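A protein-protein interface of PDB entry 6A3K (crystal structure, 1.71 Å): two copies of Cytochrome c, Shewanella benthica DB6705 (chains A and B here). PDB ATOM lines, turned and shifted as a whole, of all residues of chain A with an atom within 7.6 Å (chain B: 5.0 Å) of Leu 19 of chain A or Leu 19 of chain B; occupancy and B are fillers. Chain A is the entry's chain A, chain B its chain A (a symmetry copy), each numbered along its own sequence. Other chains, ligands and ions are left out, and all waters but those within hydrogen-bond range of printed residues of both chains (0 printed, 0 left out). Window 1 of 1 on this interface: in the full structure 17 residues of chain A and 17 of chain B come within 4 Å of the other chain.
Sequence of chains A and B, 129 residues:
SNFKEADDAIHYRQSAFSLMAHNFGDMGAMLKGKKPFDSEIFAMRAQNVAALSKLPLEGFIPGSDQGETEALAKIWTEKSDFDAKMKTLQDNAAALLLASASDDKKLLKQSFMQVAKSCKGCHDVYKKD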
ATOM      1  N   PHE A   3      -1.975 -43.832  24.939  1.00  0.00           N
ATOM      2  CA  PHE A   3      -0.991 -43.204  25.817  1.00  0.00           C
ATOM      3  C   PHE A   3       0.203 -44.123  26.038  1.00  0.00           C
ATOM      4  O   PHE A   3       0.048 -45.346  26.134  1.00  0.00           O
ATOM      5  CB  PHE A   3      -1.608 -42.857  27.170  1.00  0.00           C
ATOM      6  CG  PHE A   3      -2.810 -41.967  27.072  1.00  0.00           C
ATOM      7  CD1 PHE A   3      -2.669 -40.586  27.065  1.00  0.00           C
ATOM      8  CD2 PHE A   3      -4.082 -42.511  26.981  1.00  0.00           C
ATOM      9  CE1 PHE A   3      -3.792 -39.766  26.976  1.00  0.00           C
ATOM     10  CE2 PHE A   3      -5.200 -41.700  26.904  1.00  0.00           C
ATOM     11  CZ  PHE A   3      -5.056 -40.335  26.895  1.00  0.00           C
ATOM     12  N   ASP A   8       0.518 -40.682  31.699  1.00  0.00           N
ATOM     13  CA  ASP A   8       0.140 -39.774  30.616  1.00  0.00           C
ATOM     14  C   ASP A   8      -1.371 -39.674  30.486  1.00  0.00           C
ATOM     15  O   ASP A   8      -1.907 -38.603  30.172  1.00  0.00           O
ATOM     16  CB  ASP A   8       0.732 -40.244  29.289  1.00  0.00           C
ATOM     17  CG  ASP A   8       2.241 -40.209  29.279  1.00  0.00           C
ATOM     18  OD1 ASP A   8       2.817 -39.275  29.867  1.00  0.00           O
ATOM     19  OD2 ASP A   8       2.845 -41.127  28.692  1.00  0.00           O
ATOM     20  N   HIS A  11      -2.533 -37.497  33.473  1.00  0.00           N
ATOM     21  CA  HIS A  11      -2.275 -36.083  33.232  1.00  0.00           C
ATOM     22  C   HIS A  11      -3.250 -35.512  32.202  1.00  0.00           C
ATOM     23  O   HIS A  11      -3.738 -34.388  32.358  1.00  0.00           O
ATOM     24  CB  HIS A  11      -0.830 -35.914  32.770  1.00  0.00           C
ATOM     25  CG  HIS A  11      -0.522 -34.546  32.253  1.00  0.00           C
ATOM     26  ND1 HIS A  11      -0.207 -33.492  33.083  1.00  0.00           N
ATOM     27  CD2 HIS A  11      -0.481 -34.057  30.990  1.00  0.00           C
ATOM     28  CE1 HIS A  11       0.017 -32.413  32.354  1.00  0.00           C
ATOM     29  NE2 HIS A  11      -0.142 -32.729  31.081  1.00  0.00           N
ATOM     30  N   TYR A  12      -3.536 -36.275  31.141  1.00  0.00           N
ATOM     31  CA  TYR A  12      -4.464 -35.819  30.103  1.00  0.00           C
ATOM     32  C   TYR A  12      -5.843 -35.507  30.686  1.00  0.00           C
ATOM     33  O   TYR A  12      -6.360 -34.395  30.525  1.00  0.00           O
ATOM     34  CB  TYR A  12      -4.574 -36.879  28.994  1.00  0.00           C
ATOM     35  CG  TYR A  12      -5.423 -36.450  27.807  1.00  0.00           C
ATOM     36  CD1 TYR A  12      -4.862 -35.752  26.746  1.00  0.00           C
ATOM     37  CD2 TYR A  12      -6.772 -36.778  27.737  1.00  0.00           C
ATOM     38  CE1 TYR A  12      -5.626 -35.352  25.667  1.00  0.00           C
ATOM     39  CE2 TYR A  12      -7.548 -36.388  26.653  1.00  0.00           C
ATOM     40  CZ  TYR A  12      -6.954 -35.680  25.617  1.00  0.00           C
ATOM     41  OH  TYR A  12      -7.706 -35.278  24.547  1.00  0.00           O
ATOM     42  N   ARG A  13      -6.450 -36.467  31.382  1.00  0.00           N
ATOM     43  CA  ARG A  13      -7.794 -36.213  31.903  1.00  0.00           C
ATOM     44  C   ARG A  13      -7.774 -35.101  32.950  1.00  0.00           C
ATOM     45  O   ARG A  13      -8.650 -34.231  32.954  1.00  0.00           O
ATOM     46  CB  ARG A  13      -8.413 -37.502  32.455  1.00  0.00           C
ATOM     47  CG  ARG A  13      -7.758 -38.091  33.717  1.00  0.00           C
ATOM     48  CD  ARG A  13      -7.966 -39.609  33.785  1.00  0.00           C
ATOM     49  NE  ARG A  13      -7.639 -40.179  35.101  1.00  0.00           N
ATOM     50  CZ  ARG A  13      -7.312 -41.454  35.312  1.00  0.00           C
ATOM     51  NH1 ARG A  13      -7.228 -42.294  34.291  1.00  0.00           N
ATOM     52  NH2 ARG A  13      -7.065 -41.892  36.551  1.00  0.00           N
ATOM     53  N   GLN A  14      -6.766 -35.087  33.822  1.00  0.00           N
ATOM     54  CA  GLN A  14      -6.665 -34.006  34.797  1.00  0.00           C
ATOM     55  C   GLN A  14      -6.543 -32.652  34.113  1.00  0.00           C
ATOM     56  O   GLN A  14      -7.189 -31.686  34.525  1.00  0.00           O
ATOM     57  CB  GLN A  14      -5.481 -34.244  35.731  1.00  0.00           C
ATOM     58  CG  GLN A  14      -5.715 -35.373  36.711  1.00  0.00           C
ATOM     59  CD  GLN A  14      -4.536 -35.594  37.622  1.00  0.00           C
ATOM     60  OE1 GLN A  14      -3.416 -35.165  37.317  1.00  0.00           O
ATOM     61  NE2 GLN A  14      -4.773 -36.267  38.749  1.00  0.00           N
ATOM     62  N   SER A  15      -5.739 -32.560  33.051  1.00  0.00           N
ATOM     63  CA  SER A  15      -5.592 -31.277  32.371  1.00  0.00           C
ATOM     64  C   SER A  15      -6.904 -30.835  31.731  1.00  0.00           C
ATOM     65  O   SER A  15      -7.253 -29.654  31.791  1.00  0.00           O
ATOM     66  CB  SER A  15      -4.490 -31.356  31.318  1.00  0.00           C
ATOM     67  OG  SER A  15      -3.222 -31.457  31.939  1.00  0.00           O
ATOM     68  N   ALA A  16      -7.642 -31.767  31.126  1.00  0.00           N
ATOM     69  CA  ALA A  16      -8.902 -31.394  30.492  1.00  0.00           C
ATOM     70  C   ALA A  16      -9.893 -30.896  31.530  1.00  0.00           C
ATOM     71  O   ALA A  16     -10.561 -29.878  31.320  1.00  0.00           O
ATOM     72  CB  ALA A  16      -9.490 -32.570  29.712  1.00  0.00           C
ATOM     73  N   PHE A  17      -9.986 -31.591  32.669  1.00  0.00           N
ATOM     74  CA  PHE A  17     -10.878 -31.140  33.738  1.00  0.00           C
ATOM     75  C   PHE A  17     -10.475 -29.765  34.253  1.00  0.00           C
ATOM     76  O   PHE A  17     -11.332 -28.911  34.508  1.00  0.00           O
ATOM     77  CB  PHE A  17     -10.864 -32.145  34.884  1.00  0.00           C
ATOM     78  CG  PHE A  17     -11.628 -33.398  34.601  1.00  0.00           C
ATOM     79  CD1 PHE A  17     -12.935 -33.353  34.131  1.00  0.00           C
ATOM     80  CD2 PHE A  17     -11.044 -34.636  34.826  1.00  0.00           C
ATOM     81  CE1 PHE A  17     -13.637 -34.533  33.895  1.00  0.00           C
ATOM     82  CE2 PHE A  17     -11.740 -35.798  34.592  1.00  0.00           C
ATOM     83  CZ  PHE A  17     -13.041 -35.745  34.125  1.00  0.00           C
ATOM     84  N   SER A  18      -9.179 -29.544  34.464  1.00  0.00           N
ATOM     85  CA  SER A  18      -8.725 -28.245  34.949  1.00  0.00           C
ATOM     86  C   SER A  18      -9.110 -27.127  33.984  1.00  0.00           C
ATOM     87  O   SER A  18      -9.600 -26.072  34.406  1.00  0.00           O
ATOM     88  CB  SER A  18      -7.209 -28.286  35.175  1.00  0.00           C
ATOM     89  OG  SER A  18      -6.713 -27.022  35.581  1.00  0.00           O
ATOM     90  N   LEU A  19      -8.910 -27.341  32.678  1.00  0.00           N
ATOM     91  CA  LEU A  19      -9.306 -26.319  31.711  1.00  0.00           C
ATOM     92  C   LEU A  19     -10.819 -26.121  31.713  1.00  0.00           C
ATOM     93  O   LEU A  19     -11.304 -24.989  31.569  1.00  0.00           O
ATOM     94  CB  LEU A  19      -8.821 -26.692  30.312  1.00  0.00           C
ATOM     95  CG  LEU A  19      -7.308 -26.746  30.083  1.00  0.00           C
ATOM     96  CD1 LEU A  19      -7.001 -27.154  28.651  1.00  0.00           C
ATOM     97  CD2 LEU A  19      -6.689 -25.422  30.369  1.00  0.00           C
ATOM     98  N   MET A  20     -11.581 -27.212  31.854  1.00  0.00           N
ATOM     99  CA  MET A  20     -13.038 -27.110  31.947  1.00  0.00           C
ATOM    100  C   MET A  20     -13.441 -26.232  33.119  1.00  0.00           C
ATOM    101  O   MET A  20     -14.309 -25.362  33.000  1.00  0.00           O
ATOM    102  CB  MET A  20     -13.663 -28.497  32.125  1.00  0.00           C
ATOM    103  CG  MET A  20     -13.617 -29.382  30.913  1.00  0.00           C
ATOM    104  SD  MET A  20     -13.867 -31.130  31.281  1.00  0.00           S
ATOM    105  CE  MET A  20     -15.483 -31.122  32.050  1.00  0.00           C
ATOM    106  N   ALA A  21     -12.809 -26.462  34.275  1.00  0.00           N
ATOM    107  CA  ALA A  21     -13.153 -25.715  35.476  1.00  0.00           C
ATOM    108  C   ALA A  21     -12.861 -24.229  35.314  1.00  0.00           C
ATOM    109  O   ALA A  21     -13.623 -23.386  35.793  1.00  0.00           O
ATOM    110  CB  ALA A  21     -12.403 -26.282  36.680  1.00  0.00           C
ATOM    111  N   HIS A  22     -11.762 -23.876  34.652  1.00  0.00           N
ATOM    112  CA  HIS A  22     -11.482 -22.453  34.481  1.00  0.00           C
ATOM    113  C   HIS A  22     -12.586 -21.797  33.667  1.00  0.00           C
ATOM    114  O   HIS A  22     -13.097 -20.727  34.028  1.00  0.00           O
ATOM    115  CB  HIS A  22     -10.129 -22.227  33.800  1.00  0.00           C
ATOM    116  CG  HIS A  22      -9.870 -20.787  33.455  1.00  0.00           C
ATOM    117  ND1 HIS A  22      -9.513 -19.847  34.399  1.00  0.00           N
ATOM    118  CD2 HIS A  22      -9.954 -20.120  32.278  1.00  0.00           C
ATOM    119  CE1 HIS A  22      -9.369 -18.670  33.815  1.00  0.00           C
ATOM    120  NE2 HIS A  22      -9.637 -18.807  32.529  1.00  0.00           N
ATOM    121  N   ASN A  23     -12.981 -22.442  32.574  1.00  0.00           N
ATOM    122  CA  ASN A  23     -13.976 -21.836  31.699  1.00  0.00           C
ATOM    123  C   ASN A  23     -15.348 -21.846  32.352  1.00  0.00           C
ATOM    124  O   ASN A  23     -16.079 -20.855  32.273  1.00  0.00           O
ATOM    125  CB  ASN A  23     -14.005 -22.561  30.358  1.00  0.00           C
ATOM    126  CG  ASN A  23     -12.835 -22.168  29.481  1.00  0.00           C
ATOM    127  OD1 ASN A  23     -12.902 -21.170  28.765  1.00  0.00           O
ATOM    128  ND2 ASN A  23     -11.749 -22.937  29.550  1.00  0.00           N
ATOM    129  N   PHE A  24     -15.707 -22.957  32.999  1.00  0.00           N
ATOM    130  CA  PHE A  24     -17.003 -23.054  33.666  1.00  0.00           C
ATOM    131  C   PHE A  24     -17.117 -22.060  34.818  1.00  0.00           C
ATOM    132  O   PHE A  24     -18.177 -21.453  35.030  1.00  0.00           O
ATOM    133  CB  PHE A  24     -17.205 -24.482  34.181  1.00  0.00           C
ATOM    134  CG  PHE A  24     -18.617 -24.789  34.572  1.00  0.00           C
ATOM    135  CD1 PHE A  24     -19.640 -24.723  33.632  1.00  0.00           C
ATOM    136  CD2 PHE A  24     -18.918 -25.155  35.877  1.00  0.00           C
ATOM    137  CE1 PHE A  24     -20.956 -25.007  33.994  1.00  0.00           C
ATOM    138  CE2 PHE A  24     -20.229 -25.446  36.247  1.00  0.00           C
ATOM    139  CZ  PHE A  24     -21.244 -25.377  35.293  1.00  0.00           C
ATOM    140  N   GLY A  25     -16.052 -21.907  35.597  1.00  0.00           N
ATOM    141  CA  GLY A  25     -16.097 -20.978  36.715  1.00  0.00           C
ATOM    142  C   GLY A  25     -16.237 -19.527  36.296  1.00  0.00           C
ATOM    143  O   GLY A  25     -16.801 -18.716  37.029  1.00  0.00           O
ATOM    144  N   ARG A  45     -17.006 -18.956  26.568  1.00  0.00           N
ATOM    145  CA  ARG A  45     -16.791 -19.945  27.619  1.00  0.00           C
ATOM    146  C   ARG A  45     -17.648 -21.186  27.397  1.00  0.00           C
ATOM    147  O   ARG A  45     -17.181 -22.315  27.597  1.00  0.00           O
ATOM    148  CB  ARG A  45     -17.101 -19.343  28.990  1.00  0.00           C
ATOM    149  CG  ARG A  45     -16.241 -18.166  29.415  1.00  0.00           C
ATOM    150  CD  ARG A  45     -14.756 -18.534  29.527  1.00  0.00           C
ATOM    151  NE  ARG A  45     -13.953 -17.421  30.035  1.00  0.00           N
ATOM    152  CZ  ARG A  45     -12.625 -17.369  29.976  1.00  0.00           C
ATOM    153  NH1 ARG A  45     -11.956 -18.368  29.413  1.00  0.00           N
ATOM    154  NH2 ARG A  45     -11.969 -16.316  30.457  1.00  0.00           N
ATOM    155  N   ASN A  48     -16.079 -23.323  24.831  1.00  0.00           N
ATOM    156  CA  ASN A  48     -14.907 -24.002  25.369  1.00  0.00           C
ATOM    157  C   ASN A  48     -15.299 -25.158  26.280  1.00  0.00           C
ATOM    158  O   ASN A  48     -14.704 -26.233  26.209  1.00  0.00           O
ATOM    159  CB  ASN A  48     -14.027 -23.005  26.120  1.00  0.00           C
ATOM    160  CG  ASN A  48     -13.406 -21.977  25.206  1.00  0.00           C
ATOM    161  OD1 ASN A  48     -13.380 -22.151  23.980  1.00  0.00           O
ATOM    162  ND2 ASN A  48     -12.886 -20.911  25.788  1.00  0.00           N
ATOM    163  N   VAL A  49     -16.301 -24.962  27.146  1.00  0.00           N
ATOM    164  CA  VAL A  49     -16.700 -26.053  28.035  1.00  0.00           C
ATOM    165  C   VAL A  49     -17.255 -27.231  27.238  1.00  0.00           C
ATOM    166  O   VAL A  49     -17.007 -28.399  27.563  1.00  0.00           O
ATOM    167  CB  VAL A  49     -17.713 -25.543  29.082  1.00  0.00           C
ATOM    168  CG1 VAL A  49     -18.358 -26.721  29.832  1.00  0.00           C
ATOM    169  CG2 VAL A  49     -17.002 -24.611  30.052  1.00  0.00           C
ATOM    170  N   LEU A  52     -14.216 -28.938  25.561  1.00  0.00           N
ATOM    171  CA  LEU A  52     -13.374 -29.615  26.544  1.00  0.00           C
ATOM    172  C   LEU A  52     -14.061 -30.828  27.154  1.00  0.00           C
ATOM    173  O   LEU A  52     -13.390 -31.792  27.519  1.00  0.00           O
ATOM    174  CB  LEU A  52     -12.984 -28.644  27.640  1.00  0.00           C
ATOM    175  CG  LEU A  52     -11.966 -27.594  27.217  1.00  0.00           C
ATOM    176  CD1 LEU A  52     -12.042 -26.409  28.160  1.00  0.00           C
ATOM    177  CD2 LEU A  52     -10.589 -28.220  27.251  1.00  0.00           C
ATOM    178  N   LEU A  55     -13.240 -34.318  25.948  1.00  0.00           N
ATOM    179  CA  LEU A  55     -11.860 -34.806  26.000  1.00  0.00           C
ATOM    180  C   LEU A  55     -11.546 -35.822  27.102  1.00  0.00           C
ATOM    181  O   LEU A  55     -10.816 -36.780  26.828  1.00  0.00           O
ATOM    182  CB  LEU A  55     -10.882 -33.635  26.146  1.00  0.00           C
ATOM    183  CG  LEU A  55     -10.923 -32.593  25.028  1.00  0.00           C
ATOM    184  CD1 LEU A  55      -9.821 -31.562  25.233  1.00  0.00           C
ATOM    185  CD2 LEU A  55     -10.812 -33.293  23.679  1.00  0.00           C
ATOM    186  N   PRO A  56     -12.002 -35.659  28.355  1.00  0.00           N
ATOM    187  CA  PRO A  56     -11.381 -36.449  29.443  1.00  0.00           C
ATOM    188  C   PRO A  56     -11.701 -37.939  29.447  1.00  0.00           C
ATOM    189  O   PRO A  56     -10.911 -38.702  30.028  1.00  0.00           O
ATOM    190  CB  PRO A  56     -11.909 -35.779  30.721  1.00  0.00           C
ATOM    191  CG  PRO A  56     -13.166 -35.129  30.319  1.00  0.00           C
ATOM    192  CD  PRO A  56     -12.918 -34.637  28.909  1.00  0.00           C
ATOM    193  N   TYR B  12      -2.678 -23.057  33.069  1.00  0.00           N
ATOM    194  CA  TYR B  12      -3.721 -23.083  32.041  1.00  0.00           C
ATOM    195  C   TYR B  12      -3.120 -23.226  30.642  1.00  0.00           C
ATOM    196  O   TYR B  12      -3.468 -24.149  29.896  1.00  0.00           O
ATOM    197  CB  TYR B  12      -4.582 -21.812  32.133  1.00  0.00           C
ATOM    198  CG  TYR B  12      -5.770 -21.797  31.184  1.00  0.00           C
ATOM    199  CD1 TYR B  12      -6.987 -22.352  31.557  1.00  0.00           C
ATOM    200  CD2 TYR B  12      -5.679 -21.195  29.934  1.00  0.00           C
ATOM    201  CE1 TYR B  12      -8.069 -22.349  30.699  1.00  0.00           C
ATOM    202  CE2 TYR B  12      -6.764 -21.179  29.066  1.00  0.00           C
ATOM    203  CZ  TYR B  12      -7.961 -21.756  29.471  1.00  0.00           C
ATOM    204  OH  TYR B  12      -9.036 -21.759  28.625  1.00  0.00           O
ATOM    205  N   SER B  15      -1.416 -26.567  30.174  1.00  0.00           N
ATOM    206  CA  SER B  15      -2.350 -27.678  30.027  1.00  0.00           C
ATOM    207  C   SER B  15      -2.975 -27.697  28.636  1.00  0.00           C
ATOM    208  O   SER B  15      -3.132 -28.768  28.045  1.00  0.00           O
ATOM    209  CB  SER B  15      -3.439 -27.602  31.096  1.00  0.00           C
ATOM    210  OG  SER B  15      -2.898 -27.895  32.370  1.00  0.00           O
ATOM    211  N   ALA B  16      -3.327 -26.529  28.099  1.00  0.00           N
ATOM    212  CA  ALA B  16      -3.936 -26.494  26.773  1.00  0.00           C
ATOM    213  C   ALA B  16      -2.955 -26.990  25.725  1.00  0.00           C
ATOM    214  O   ALA B  16      -3.321 -27.783  24.850  1.00  0.00           O
ATOM    215  CB  ALA B  16      -4.418 -25.085  26.431  1.00  0.00           C
ATOM    216  N   PHE B  17      -1.695 -26.550  25.810  1.00  0.00           N
ATOM    217  CA  PHE B  17      -0.682 -27.027  24.868  1.00  0.00           C
ATOM    218  C   PHE B  17      -0.485 -28.532  24.981  1.00  0.00           C
ATOM    219  O   PHE B  17      -0.350 -29.229  23.969  1.00  0.00           O
ATOM    220  CB  PHE B  17       0.641 -26.313  25.123  1.00  0.00           C
ATOM    221  CG  PHE B  17       0.671 -24.900  24.638  1.00  0.00           C
ATOM    222  CD1 PHE B  17       0.293 -24.578  23.340  1.00  0.00           C
ATOM    223  CD2 PHE B  17       1.102 -23.883  25.476  1.00  0.00           C
ATOM    224  CE1 PHE B  17       0.349 -23.257  22.899  1.00  0.00           C
ATOM    225  CE2 PHE B  17       1.158 -22.582  25.039  1.00  0.00           C
ATOM    226  CZ  PHE B  17       0.780 -22.269  23.745  1.00  0.00           C
ATOM    227  N   SER B  18      -0.413 -29.051  26.206  1.00  0.00           N
ATOM    228  CA  SER B  18      -0.233 -30.489  26.385  1.00  0.00           C
ATOM    229  C   SER B  18      -1.377 -31.274  25.747  1.00  0.00           C
ATOM    230  O   SER B  18      -1.145 -32.272  25.054  1.00  0.00           O
ATOM    231  CB  SER B  18      -0.108 -30.805  27.879  1.00  0.00           C
ATOM    232  OG  SER B  18      -0.002 -32.200  28.105  1.00  0.00           O
ATOM    233  N   LEU B  19      -2.622 -30.832  25.956  1.00  0.00           N
ATOM    234  CA  LEU B  19      -3.747 -31.522  25.329  1.00  0.00           C
ATOM    235  C   LEU B  19      -3.682 -31.405  23.809  1.00  0.00           C
ATOM    236  O   LEU B  19      -4.019 -32.358  23.091  1.00  0.00           O
ATOM    237  CB  LEU B  19      -5.071 -30.966  25.848  1.00  0.00           C
ATOM    238  CG  LEU B  19      -5.388 -31.173  27.331  1.00  0.00           C
ATOM    239  CD1 LEU B  19      -6.724 -30.540  27.684  1.00  0.00           C
ATOM    240  CD2 LEU B  19      -5.419 -32.625  27.662  1.00  0.00           C
ATOM    241  N   MET B  20      -3.271 -30.237  23.300  1.00  0.00           N
ATOM    242  CA  MET B  20      -3.101 -30.059  21.857  1.00  0.00           C
ATOM    243  C   MET B  20      -2.107 -31.065  21.305  1.00  0.00           C
ATOM    244  O   MET B  20      -2.340 -31.696  20.269  1.00  0.00           O
ATOM    245  CB  MET B  20      -2.603 -28.645  21.546  1.00  0.00           C
ATOM    246  CG  MET B  20      -3.610 -27.550  21.750  1.00  0.00           C
ATOM    247  SD  MET B  20      -2.879 -25.906  21.887  1.00  0.00           S
ATOM    248  CE  MET B  20      -2.018 -25.750  20.325  1.00  0.00           C
ATOM    249  N   ALA B  21      -0.974 -31.221  21.999  1.00  0.00           N
ATOM    250  CA  ALA B  21       0.072 -32.120  21.534  1.00  0.00           C
ATOM    251  C   ALA B  21      -0.408 -33.565  21.498  1.00  0.00           C
ATOM    252  O   ALA B  21      -0.060 -34.318  20.586  1.00  0.00           O
ATOM    253  CB  ALA B  21       1.311 -31.986  22.416  1.00  0.00           C
ATOM    254  N   HIS B  22      -1.202 -33.985  22.481  1.00  0.00           N
ATOM    255  CA  HIS B  22      -1.677 -35.365  22.447  1.00  0.00           C
ATOM    256  C   HIS B  22      -2.530 -35.595  21.209  1.00  0.00           C
ATOM    257  O   HIS B  22      -2.359 -36.590  20.491  1.00  0.00           O
ATOM    258  CB  HIS B  22      -2.482 -35.711  23.704  1.00  0.00           C
ATOM    259  CG  HIS B  22      -3.128 -37.067  23.643  1.00  0.00           C
ATOM    260  ND1 HIS B  22      -2.422 -38.238  23.814  1.00  0.00           N
ATOM    261  CD2 HIS B  22      -4.408 -37.436  23.390  1.00  0.00           C
ATOM    262  CE1 HIS B  22      -3.240 -39.268  23.690  1.00  0.00           C
ATOM    263  NE2 HIS B  22      -4.451 -38.809  23.426  1.00  0.00           N
ATOM    264  N   ASN B  23      -3.439 -34.665  20.935  1.00  0.00           N
ATOM    265  CA  ASN B  23      -4.350 -34.857  19.813  1.00  0.00           C
ATOM    266  C   ASN B  23      -3.615 -34.708  18.491  1.00  0.00           C
ATOM    267  O   ASN B  23      -3.843 -35.490  17.563  1.00  0.00           O
ATOM    268  CB  ASN B  23      -5.510 -33.872  19.906  1.00  0.00           C
ATOM    269  CG  ASN B  23      -6.527 -34.298  20.944  1.00  0.00           C
ATOM    270  OD1 ASN B  23      -7.424 -35.086  20.648  1.00  0.00           O
ATOM    271  ND2 ASN B  23      -6.377 -33.799  22.170  1.00  0.00           N
ATOM    272  N   LEU B  52      -8.887 -26.714  20.941  1.00  0.00           N
ATOM    273  CA  LEU B  52      -7.846 -26.447  21.931  1.00  0.00           C
ATOM    274  C   LEU B  52      -6.958 -25.278  21.533  1.00  0.00           C
ATOM    275  O   LEU B  52      -6.452 -24.570  22.403  1.00  0.00           O
ATOM    276  CB  LEU B  52      -7.000 -27.687  22.132  1.00  0.00           C
ATOM    277  CG  LEU B  52      -7.696 -28.807  22.893  1.00  0.00           C
ATOM    278  CD1 LEU B  52      -7.011 -30.125  22.589  1.00  0.00           C
ATOM    279  CD2 LEU B  52      -7.630 -28.495  24.372  1.00  0.00           C
ATOM    280  N   LEU B  55      -7.483 -21.852  23.048  1.00  0.00           N
ATOM    281  CA  LEU B  55      -7.428 -21.677  24.502  1.00  0.00           C
ATOM    282  C   LEU B  55      -6.167 -21.004  25.052  1.00  0.00           C
ATOM    283  O   LEU B  55      -6.290 -20.178  25.962  1.00  0.00           O
ATOM    284  CB  LEU B  55      -7.590 -23.025  25.211  1.00  0.00           C
ATOM    285  CG  LEU B  55      -8.891 -23.775  24.922  1.00  0.00           C
ATOM    286  CD1 LEU B  55      -8.976 -25.028  25.785  1.00  0.00           C
ATOM    287  CD2 LEU B  55     -10.074 -22.841  25.147  1.00  0.00           C
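Of the printed residues of chain B, Leu 19 of chain A touches Tyr 12 (3.3 Å), Ser 15 (3.98 Å), Ala 16 (3.7 Å) and Leu 19 (3.5 Å). Leu 19 of chain B touches just these residues of chain A: Tyr 12, Ser 15, Ala 16 and Leu 19. Of the printed residues of chain A, Ser 15 of chain B touches Ser 15 (3.6 Å) and Leu 19 (3.98 Å). Of the printed residues of chain B, Phe 3 of chain A touches His 22 (3.4 Å). Of the printed residues of chain B, Ala 16 of chain A touches Leu 19 (3.7 Å). Of the printed residues of chain B, Leu 52 of chain A touches Leu 55 (3.9 Å). Ser 18 of chain A touches none of the printed residues of chain B. Ala 21 of chain B touches none of the printed residues of chain A. The nearest residue of chain A that does not touch Leu 19 of chain B is Leu 55 of chain A (4.1 Å). The nearest printed residue of chain A that does not touch Asn 23 of chain B is Leu 55 of chain A (4.7 Å).
Among the printed residues, pairs that only touch across the chains: Leu 19 of chain A with Tyr 12 of chain B (3.3 Å), Tyr 12 of chain A with Leu 19 of chain B (3.3 Å), Tyr 12 of chain A with His 22 of chain B (3.3 Å), His 22 of chain A with Tyr 12 of chain B (3.3 Å), Phe 3 of chain A with His 22 of chain B (3.4 Å), Asn 48 of chain A with Leu 55 of chain B (3.4 Å), Leu 19 of chain A with Leu 19 of chain B (3.5 Å), Ser 15 of chain A with Ser 15 of chain B (3.6 Å), Leu 19 of chain A with Ala 16 of chain B (3.7 Å), Ala 16 of chain A with Leu 19 of chain B (3.7 Å), Leu 52 of chain A with Leu 55 of chain B (3.9 Å), Leu 55 of chain A with Leu 52 of chain B (3.9 Å), Ser 15 of chain A with Leu 19 of chain B (3.98 Å) and Leu 19 of chain A with Ser 15 of chain B (3.98 Å).
Of the 12 printed residues of chain B, 9 touch a printed residue of chain A. Printed residues of chain B that touch a printed residue of chain A: Tyr 12, Ser 15, Ala 16, Ser 18, Leu 19, His 22, Asn 23, Leu 52 and Leu 55. Hydrophobic or aromatic side chains of chain A that line the printed part of chain B: Phe 3, His 11, Tyr 12, Ala 16, Leu 19, His 22, Leu 52 and Leu 55.
Tyr 12 of chain A touches Leu 19 of chain B, and with the chains exchanged Leu 19 of chain A touches Tyr 12 of chain B. Ser 15 of chain A touches its own counterpart, Ser 15 of chain B. Ala 16 of chain A touches Leu 19 of chain B, and with the chains exchanged Leu 19 of chain A touches Ala 16 of chain B. Leu 52 of chain A touches Leu 55 of chain B, and with the chains exchanged Leu 55 of chain A touches Leu 52 of chain B.
The side-chain hydroxyl (OH) of Tyr 12 of chain A sits at hydrogen-bond distance from the side-chain amide nitrogen (ND2) of Asn 23 of chain B, 3.1 Å away. The side-chain hydroxyl (OG) of Ser 18 of chain B sits at hydrogen-bond distance from a ring nitrogen (NE2) of His 11 of chain A (3.0 Å). ND2 of Asn 23 of chain A sits at hydrogen-bond distance from OH of Tyr 12 of chain B, 3.1 Å away.
O of Leu 19 of chain B is in hydrogen-bond range of ND2 of Asn 23 of chain B, 2.9 Å away. The side-chain hydroxyl (OG) of Ser 15 of chain A sits at hydrogen-bond distance from the backbone carbonyl oxygen (O) of His 11 of chain A, 3.0 Å away. The side-chain amide oxygen of Asn 23 of chain A is in hydrogen-bond range of the guanidinium group of Arg 45 of chain A, at 3.0 Å. ND2 of Asn 23 of chain A is in hydrogen-bond range of O of Leu 19 of chain A (2.9 Å). The side-chain amide nitrogen (ND2) of Asn 48 of chain A is in hydrogen-bond range of the side-chain amide oxygen (OD1) of Asn 23 of chain A.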
